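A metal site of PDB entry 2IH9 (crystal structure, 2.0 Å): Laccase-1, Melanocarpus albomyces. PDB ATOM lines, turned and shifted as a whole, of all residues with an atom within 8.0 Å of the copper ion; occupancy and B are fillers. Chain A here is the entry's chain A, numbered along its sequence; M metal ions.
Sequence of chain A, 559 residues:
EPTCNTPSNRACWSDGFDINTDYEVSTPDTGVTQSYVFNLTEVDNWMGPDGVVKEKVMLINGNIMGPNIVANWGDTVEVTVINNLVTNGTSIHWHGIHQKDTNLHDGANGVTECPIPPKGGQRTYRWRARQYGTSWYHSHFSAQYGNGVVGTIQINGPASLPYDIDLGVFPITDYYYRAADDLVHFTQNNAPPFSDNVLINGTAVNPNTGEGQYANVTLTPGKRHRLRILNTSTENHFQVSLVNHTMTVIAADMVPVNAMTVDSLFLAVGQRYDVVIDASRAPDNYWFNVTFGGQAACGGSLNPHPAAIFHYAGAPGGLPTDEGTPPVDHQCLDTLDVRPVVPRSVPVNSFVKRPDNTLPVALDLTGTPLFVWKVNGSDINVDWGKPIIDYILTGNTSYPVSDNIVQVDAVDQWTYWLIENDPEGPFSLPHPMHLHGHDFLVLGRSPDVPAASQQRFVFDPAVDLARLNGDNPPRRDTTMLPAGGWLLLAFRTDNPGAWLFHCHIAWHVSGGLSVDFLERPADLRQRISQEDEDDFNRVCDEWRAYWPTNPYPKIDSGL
N of Cys 503 lies within hydrogen-bond range of O of Leu 513 (3.4 Å). The side-chain sulfur (SG) of Cys 503 sits close to the backbone NH (N) of Ile 505 (3.4 Å). O of His 508 lies within hydrogen-bond range of N of Leu 513, at 3.1 Å. The backbone carbonyl oxygen (O) of Leu 429 sits close to a ring nitrogen (NE2) of His 431, at 3.3 Å. O of His 431 is in hydrogen-bond range of N of Leu 481 (2.8 Å).
Ile 505 touches the copper ion (CD1 to CU, 3.8 Å). Leu 513 touches the copper ion (CD1 to CU, 3.8 Å). Of the 21 residues printed, 5 come within 4 Å of the copper ion. Along chain A the residues within 4 Å of the copper ion span positions 431 to 513. The nearest printed residue that does not touch the copper ion is Pro 430 (4.3 Å).
The copper ion is bound by ND1 of His 508, ND1 of His 431 and SG of Cys 503.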
ATOM      1  N   GLU A 235     -29.039  23.567  28.712  1.00  0.00           N
ATOM      2  CA  GLU A 235     -27.750  23.840  28.044  1.00  0.00           C
ATOM      3  C   GLU A 235     -27.082  22.583  27.444  1.00  0.00           C
ATOM      4  O   GLU A 235     -26.540  22.629  26.333  1.00  0.00           O
ATOM      5  CB  GLU A 235     -26.770  24.551  29.010  1.00  0.00           C
ATOM      6  CG  GLU A 235     -25.438  25.092  28.417  1.00  0.00           C
ATOM      7  CD  GLU A 235     -24.290  24.086  28.333  1.00  0.00           C
ATOM      8  OE1 GLU A 235     -24.362  23.017  28.978  1.00  0.00           O
ATOM      9  OE2 GLU A 235     -23.323  24.342  27.594  1.00  0.00           O
ATOM     10  N   HIS A 237     -25.957  19.354  25.600  1.00  0.00           N
ATOM     11  CA  HIS A 237     -26.229  18.692  24.322  1.00  0.00           C
ATOM     12  C   HIS A 237     -25.660  17.277  24.514  1.00  0.00           C
ATOM     13  O   HIS A 237     -24.494  17.107  24.892  1.00  0.00           O
ATOM     14  CB  HIS A 237     -25.526  19.388  23.169  1.00  0.00           C
ATOM     15  CG  HIS A 237     -26.025  20.767  22.872  1.00  0.00           C
ATOM     16  ND1 HIS A 237     -26.106  21.754  23.832  1.00  0.00           N
ATOM     17  CD2 HIS A 237     -26.398  21.346  21.702  1.00  0.00           C
ATOM     18  CE1 HIS A 237     -26.496  22.883  23.263  1.00  0.00           C
ATOM     19  NE2 HIS A 237     -26.680  22.661  21.972  1.00  0.00           N
ATOM     20  N   VAL A 361     -25.594  36.525  14.133  1.00  0.00           N
ATOM     21  CA  VAL A 361     -25.533  36.320  15.586  1.00  0.00           C
ATOM     22  C   VAL A 361     -24.179  36.819  16.070  1.00  0.00           C
ATOM     23  O   VAL A 361     -23.167  36.567  15.420  1.00  0.00           O
ATOM     24  CB  VAL A 361     -25.746  34.793  15.950  1.00  0.00           C
ATOM     25  CG1 VAL A 361     -25.375  34.480  17.411  1.00  0.00           C
ATOM     26  CG2 VAL A 361     -27.211  34.414  15.735  1.00  0.00           C
ATOM     27  N   TRP A 373     -26.088  38.549  23.999  1.00  0.00           N
ATOM     28  CA  TRP A 373     -26.203  37.964  22.662  1.00  0.00           C
ATOM     29  C   TRP A 373     -27.153  38.767  21.780  1.00  0.00           C
ATOM     30  O   TRP A 373     -28.324  38.955  22.115  1.00  0.00           O
ATOM     31  CB  TRP A 373     -26.662  36.502  22.761  1.00  0.00           C
ATOM     32  CG  TRP A 373     -25.660  35.576  23.363  1.00  0.00           C
ATOM     33  CD1 TRP A 373     -25.594  35.173  24.676  1.00  0.00           C
ATOM     34  CD2 TRP A 373     -24.569  34.930  22.686  1.00  0.00           C
ATOM     35  NE1 TRP A 373     -24.539  34.318  24.857  1.00  0.00           N
ATOM     36  CE2 TRP A 373     -23.889  34.148  23.660  1.00  0.00           C
ATOM     37  CE3 TRP A 373     -24.101  34.930  21.356  1.00  0.00           C
ATOM     38  CZ2 TRP A 373     -22.747  33.364  23.343  1.00  0.00           C
ATOM     39  CZ3 TRP A 373     -22.958  34.156  21.029  1.00  0.00           C
ATOM     40  CH2 TRP A 373     -22.293  33.381  22.032  1.00  0.00           C
ATOM     41  N   ASN A 421     -22.947  32.668  12.453  1.00  0.00           N
ATOM     42  CA  ASN A 421     -22.416  32.496  13.810  1.00  0.00           C
ATOM     43  C   ASN A 421     -21.139  33.282  14.168  1.00  0.00           C
ATOM     44  O   ASN A 421     -20.053  32.699  14.249  1.00  0.00           O
ATOM     45  CB  ASN A 421     -22.203  31.006  14.102  1.00  0.00           C
ATOM     46  CG  ASN A 421     -22.273  30.678  15.594  1.00  0.00           C
ATOM     47  OD1 ASN A 421     -22.339  31.566  16.435  1.00  0.00           O
ATOM     48  ND2 ASN A 421     -22.258  29.394  15.906  1.00  0.00           N
ATOM     49  N   LEU A 429     -19.435  29.840  19.685  1.00  0.00           N
ATOM     50  CA  LEU A 429     -19.950  28.631  20.298  1.00  0.00           C
ATOM     51  C   LEU A 429     -21.126  28.094  19.482  1.00  0.00           C
ATOM     52  O   LEU A 429     -21.790  28.872  18.785  1.00  0.00           O
ATOM     53  CB  LEU A 429     -20.442  28.933  21.726  1.00  0.00           C
ATOM     54  CG  LEU A 429     -19.685  29.750  22.779  1.00  0.00           C
ATOM     55  CD1 LEU A 429     -20.414  29.562  24.091  1.00  0.00           C
ATOM     56  CD2 LEU A 429     -18.245  29.317  22.940  1.00  0.00           C
ATOM     57  N   PRO A 430     -21.354  26.759  19.486  1.00  0.00           N
ATOM     58  CA  PRO A 430     -22.479  26.210  18.738  1.00  0.00           C
ATOM     59  C   PRO A 430     -23.824  26.546  19.406  1.00  0.00           C
ATOM     60  O   PRO A 430     -23.900  26.694  20.639  1.00  0.00           O
ATOM     61  CB  PRO A 430     -22.188  24.701  18.735  1.00  0.00           C
ATOM     62  CG  PRO A 430     -21.336  24.495  19.946  1.00  0.00           C
ATOM     63  CD  PRO A 430     -20.437  25.680  19.919  1.00  0.00           C
ATOM     64  N   HIS A 431     -24.860  26.755  18.584  1.00  0.00           N
ATOM     65  CA  HIS A 431     -26.190  27.118  19.085  1.00  0.00           C
ATOM     66  C   HIS A 431     -27.316  26.271  18.510  1.00  0.00           C
ATOM     67  O   HIS A 431     -27.393  26.091  17.290  1.00  0.00           O
ATOM     68  CB  HIS A 431     -26.557  28.579  18.756  1.00  0.00           C
ATOM     69  CG  HIS A 431     -25.595  29.599  19.281  1.00  0.00           C
ATOM     70  ND1 HIS A 431     -25.496  29.921  20.620  1.00  0.00           N
ATOM     71  CD2 HIS A 431     -24.675  30.356  18.646  1.00  0.00           C
ATOM     72  CE1 HIS A 431     -24.539  30.822  20.777  1.00  0.00           C
ATOM     73  NE2 HIS A 431     -24.028  31.095  19.592  1.00  0.00           N
ATOM     74  N   PRO A 432     -28.182  25.700  19.366  1.00  0.00           N
ATOM     75  CA  PRO A 432     -29.305  24.886  18.886  1.00  0.00           C
ATOM     76  C   PRO A 432     -30.475  25.810  18.511  1.00  0.00           C
ATOM     77  O   PRO A 432     -31.229  26.253  19.374  1.00  0.00           O
ATOM     78  CB  PRO A 432     -29.618  23.983  20.080  1.00  0.00           C
ATOM     79  CG  PRO A 432     -29.279  24.840  21.255  1.00  0.00           C
ATOM     80  CD  PRO A 432     -27.977  25.476  20.819  1.00  0.00           C
ATOM     81  N   MET A 433     -30.573  26.168  17.230  1.00  0.00           N
ATOM     82  CA  MET A 433     -31.625  27.069  16.759  1.00  0.00           C
ATOM     83  C   MET A 433     -32.973  26.364  16.561  1.00  0.00           C
ATOM     84  O   MET A 433     -33.070  25.365  15.826  1.00  0.00           O
ATOM     85  CB  MET A 433     -31.189  27.806  15.487  1.00  0.00           C
ATOM     86  CG  MET A 433     -29.863  28.566  15.606  1.00  0.00           C
ATOM     87  SD  MET A 433     -29.807  29.848  16.871  1.00  0.00           S
ATOM     88  CE  MET A 433     -30.913  31.067  16.179  1.00  0.00           C
ATOM     89  N   MET A 480     -28.568  22.470  14.693  1.00  0.00           N
ATOM     90  CA  MET A 480     -27.360  23.154  15.132  1.00  0.00           C
ATOM     91  C   MET A 480     -26.733  24.187  14.204  1.00  0.00           C
ATOM     92  O   MET A 480     -26.566  23.952  13.007  1.00  0.00           O
ATOM     93  CB  MET A 480     -26.269  22.136  15.466  1.00  0.00           C
ATOM     94  CG  MET A 480     -26.595  21.216  16.625  1.00  0.00           C
ATOM     95  SD  MET A 480     -26.900  22.170  18.106  1.00  0.00           S
ATOM     96  CE  MET A 480     -25.260  22.655  18.521  1.00  0.00           C
ATOM     97  N   LEU A 481     -26.396  25.327  14.787  1.00  0.00           N
ATOM     98  CA  LEU A 481     -25.707  26.405  14.086  1.00  0.00           C
ATOM     99  C   LEU A 481     -24.236  26.108  14.448  1.00  0.00           C
ATOM    100  O   LEU A 481     -23.879  26.110  15.632  1.00  0.00           O
ATOM    101  CB  LEU A 481     -26.149  27.764  14.640  1.00  0.00           C
ATOM    102  CG  LEU A 481     -25.468  29.067  14.225  1.00  0.00           C
ATOM    103  CD1 LEU A 481     -25.555  29.324  12.722  1.00  0.00           C
ATOM    104  CD2 LEU A 481     -26.058  30.244  15.002  1.00  0.00           C
ATOM    105  N   HIS A 502     -35.221  31.172  18.061  1.00  0.00           N
ATOM    106  CA  HIS A 502     -34.151  31.345  19.038  1.00  0.00           C
ATOM    107  C   HIS A 502     -33.239  30.171  19.287  1.00  0.00           C
ATOM    108  O   HIS A 502     -33.526  29.037  18.896  1.00  0.00           O
ATOM    109  CB  HIS A 502     -34.761  31.754  20.408  1.00  0.00           C
ATOM    110  CG  HIS A 502     -35.730  30.756  20.991  1.00  0.00           C
ATOM    111  ND1 HIS A 502     -35.348  29.806  21.923  1.00  0.00           N
ATOM    112  CD2 HIS A 502     -37.066  30.602  20.839  1.00  0.00           C
ATOM    113  CE1 HIS A 502     -36.406  29.122  22.310  1.00  0.00           C
ATOM    114  NE2 HIS A 502     -37.466  29.584  21.672  1.00  0.00           N
ATOM    115  N   CYS A 503     -32.154  30.459  20.003  1.00  0.00           N
ATOM    116  CA  CYS A 503     -31.196  29.461  20.460  1.00  0.00           C
ATOM    117  C   CYS A 503     -31.917  28.899  21.675  1.00  0.00           C
ATOM    118  O   CYS A 503     -32.476  29.675  22.468  1.00  0.00           O
ATOM    119  CB  CYS A 503     -29.898  30.119  20.921  1.00  0.00           C
ATOM    120  SG  CYS A 503     -28.828  29.002  21.800  1.00  0.00           S
ATOM    121  N   HIS A 504     -31.935  27.576  21.825  1.00  0.00           N
ATOM    122  CA  HIS A 504     -32.640  26.984  22.948  1.00  0.00           C
ATOM    123  C   HIS A 504     -31.840  26.876  24.252  1.00  0.00           C
ATOM    124  O   HIS A 504     -32.380  26.396  25.259  1.00  0.00           O
ATOM    125  CB  HIS A 504     -33.259  25.635  22.555  1.00  0.00           C
ATOM    126  CG  HIS A 504     -34.602  25.382  23.175  1.00  0.00           C
ATOM    127  ND1 HIS A 504     -34.771  25.091  24.513  1.00  0.00           N
ATOM    128  CD2 HIS A 504     -35.838  25.321  22.621  1.00  0.00           C
ATOM    129  CE1 HIS A 504     -36.054  24.845  24.757  1.00  0.00           C
ATOM    130  NE2 HIS A 504     -36.720  24.968  23.618  1.00  0.00           N
ATOM    131  N   ILE A 505     -30.574  27.302  24.237  1.00  0.00           N
ATOM    132  CA  ILE A 505     -29.766  27.293  25.460  1.00  0.00           C
ATOM    133  C   ILE A 505     -30.360  28.436  26.275  1.00  0.00           C
ATOM    134  O   ILE A 505     -30.357  29.603  25.832  1.00  0.00           O
ATOM    135  CB  ILE A 505     -28.230  27.526  25.224  1.00  0.00           C
ATOM    136  CG1 ILE A 505     -27.596  26.301  24.571  1.00  0.00           C
ATOM    137  CG2 ILE A 505     -27.503  27.821  26.587  1.00  0.00           C
ATOM    138  CD1 ILE A 505     -26.122  26.494  24.168  1.00  0.00           C
ATOM    139  N   ALA A 506     -30.980  28.080  27.414  1.00  0.00           N
ATOM    140  CA  ALA A 506     -31.636  29.020  28.310  1.00  0.00           C
ATOM    141  C   ALA A 506     -30.865  30.288  28.607  1.00  0.00           C
ATOM    142  O   ALA A 506     -31.416  31.370  28.547  1.00  0.00           O
ATOM    143  CB  ALA A 506     -32.029  28.344  29.605  1.00  0.00           C
ATOM    144  N   TRP A 507     -29.562  30.132  28.825  1.00  0.00           N
ATOM    145  CA  TRP A 507     -28.685  31.254  29.144  1.00  0.00           C
ATOM    146  C   TRP A 507     -28.509  32.206  27.964  1.00  0.00           C
ATOM    147  O   TRP A 507     -28.377  33.417  28.156  1.00  0.00           O
ATOM    148  CB  TRP A 507     -27.308  30.740  29.602  1.00  0.00           C
ATOM    149  CG  TRP A 507     -27.223  29.400  30.377  1.00  0.00           C
ATOM    150  CD1 TRP A 507     -26.267  28.437  30.207  1.00  0.00           C
ATOM    151  CD2 TRP A 507     -28.085  28.902  31.434  1.00  0.00           C
ATOM    152  NE1 TRP A 507     -26.466  27.381  31.067  1.00  0.00           N
ATOM    153  CE2 TRP A 507     -27.568  27.626  31.835  1.00  0.00           C
ATOM    154  CE3 TRP A 507     -29.244  29.394  32.086  1.00  0.00           C
ATOM    155  CZ2 TRP A 507     -28.163  26.849  32.845  1.00  0.00           C
ATOM    156  CZ3 TRP A 507     -29.840  28.617  33.105  1.00  0.00           C
ATOM    157  CH2 TRP A 507     -29.296  27.347  33.461  1.00  0.00           C
ATOM    158  N   HIS A 508     -28.574  31.665  26.741  1.00  0.00           N
ATOM    159  CA  HIS A 508     -28.424  32.468  25.522  1.00  0.00           C
ATOM    160  C   HIS A 508     -29.680  33.254  25.161  1.00  0.00           C
ATOM    161  O   HIS A 508     -29.584  34.468  24.941  1.00  0.00           O
ATOM    162  CB  HIS A 508     -27.931  31.611  24.345  1.00  0.00           C
ATOM    163  CG  HIS A 508     -26.531  31.102  24.532  1.00  0.00           C
ATOM    164  ND1 HIS A 508     -25.954  30.183  23.677  1.00  0.00           N
ATOM    165  CD2 HIS A 508     -25.593  31.369  25.478  1.00  0.00           C
ATOM    166  CE1 HIS A 508     -24.735  29.913  24.083  1.00  0.00           C
ATOM    167  NE2 HIS A 508     -24.486  30.610  25.178  1.00  0.00           N
ATOM    168  N   VAL A 509     -30.843  32.604  25.180  1.00  0.00           N
ATOM    169  CA  VAL A 509     -32.122  33.272  24.884  1.00  0.00           C
ATOM    170  C   VAL A 509     -32.406  34.357  25.934  1.00  0.00           C
ATOM    171  O   VAL A 509     -32.931  35.436  25.594  1.00  0.00           O
ATOM    172  CB  VAL A 509     -33.319  32.257  24.679  1.00  0.00           C
ATOM    173  CG1 VAL A 509     -33.618  31.450  25.945  1.00  0.00           C
ATOM    174  CG2 VAL A 509     -34.573  32.993  24.201  1.00  0.00           C
ATOM    175  N   LEU A 513     -30.532  36.171  22.532  1.00  0.00           N
ATOM    176  CA  LEU A 513     -30.426  35.467  21.248  1.00  0.00           C
ATOM    177  C   LEU A 513     -31.767  34.976  20.685  1.00  0.00           C
ATOM    178  O   LEU A 513     -32.078  33.777  20.782  1.00  0.00           O
ATOM    179  CB  LEU A 513     -29.438  34.293  21.336  1.00  0.00           C
ATOM    180  CG  LEU A 513     -28.553  33.992  20.112  1.00  0.00           C
ATOM    181  CD1 LEU A 513     -27.426  33.098  20.554  1.00  0.00           C
ATOM    182  CD2 LEU A 513     -29.301  33.376  18.937  1.00  0.00           C
HETATM  183 CU    CU M   1     -26.773  29.612  22.048  1.00  0.00          CU
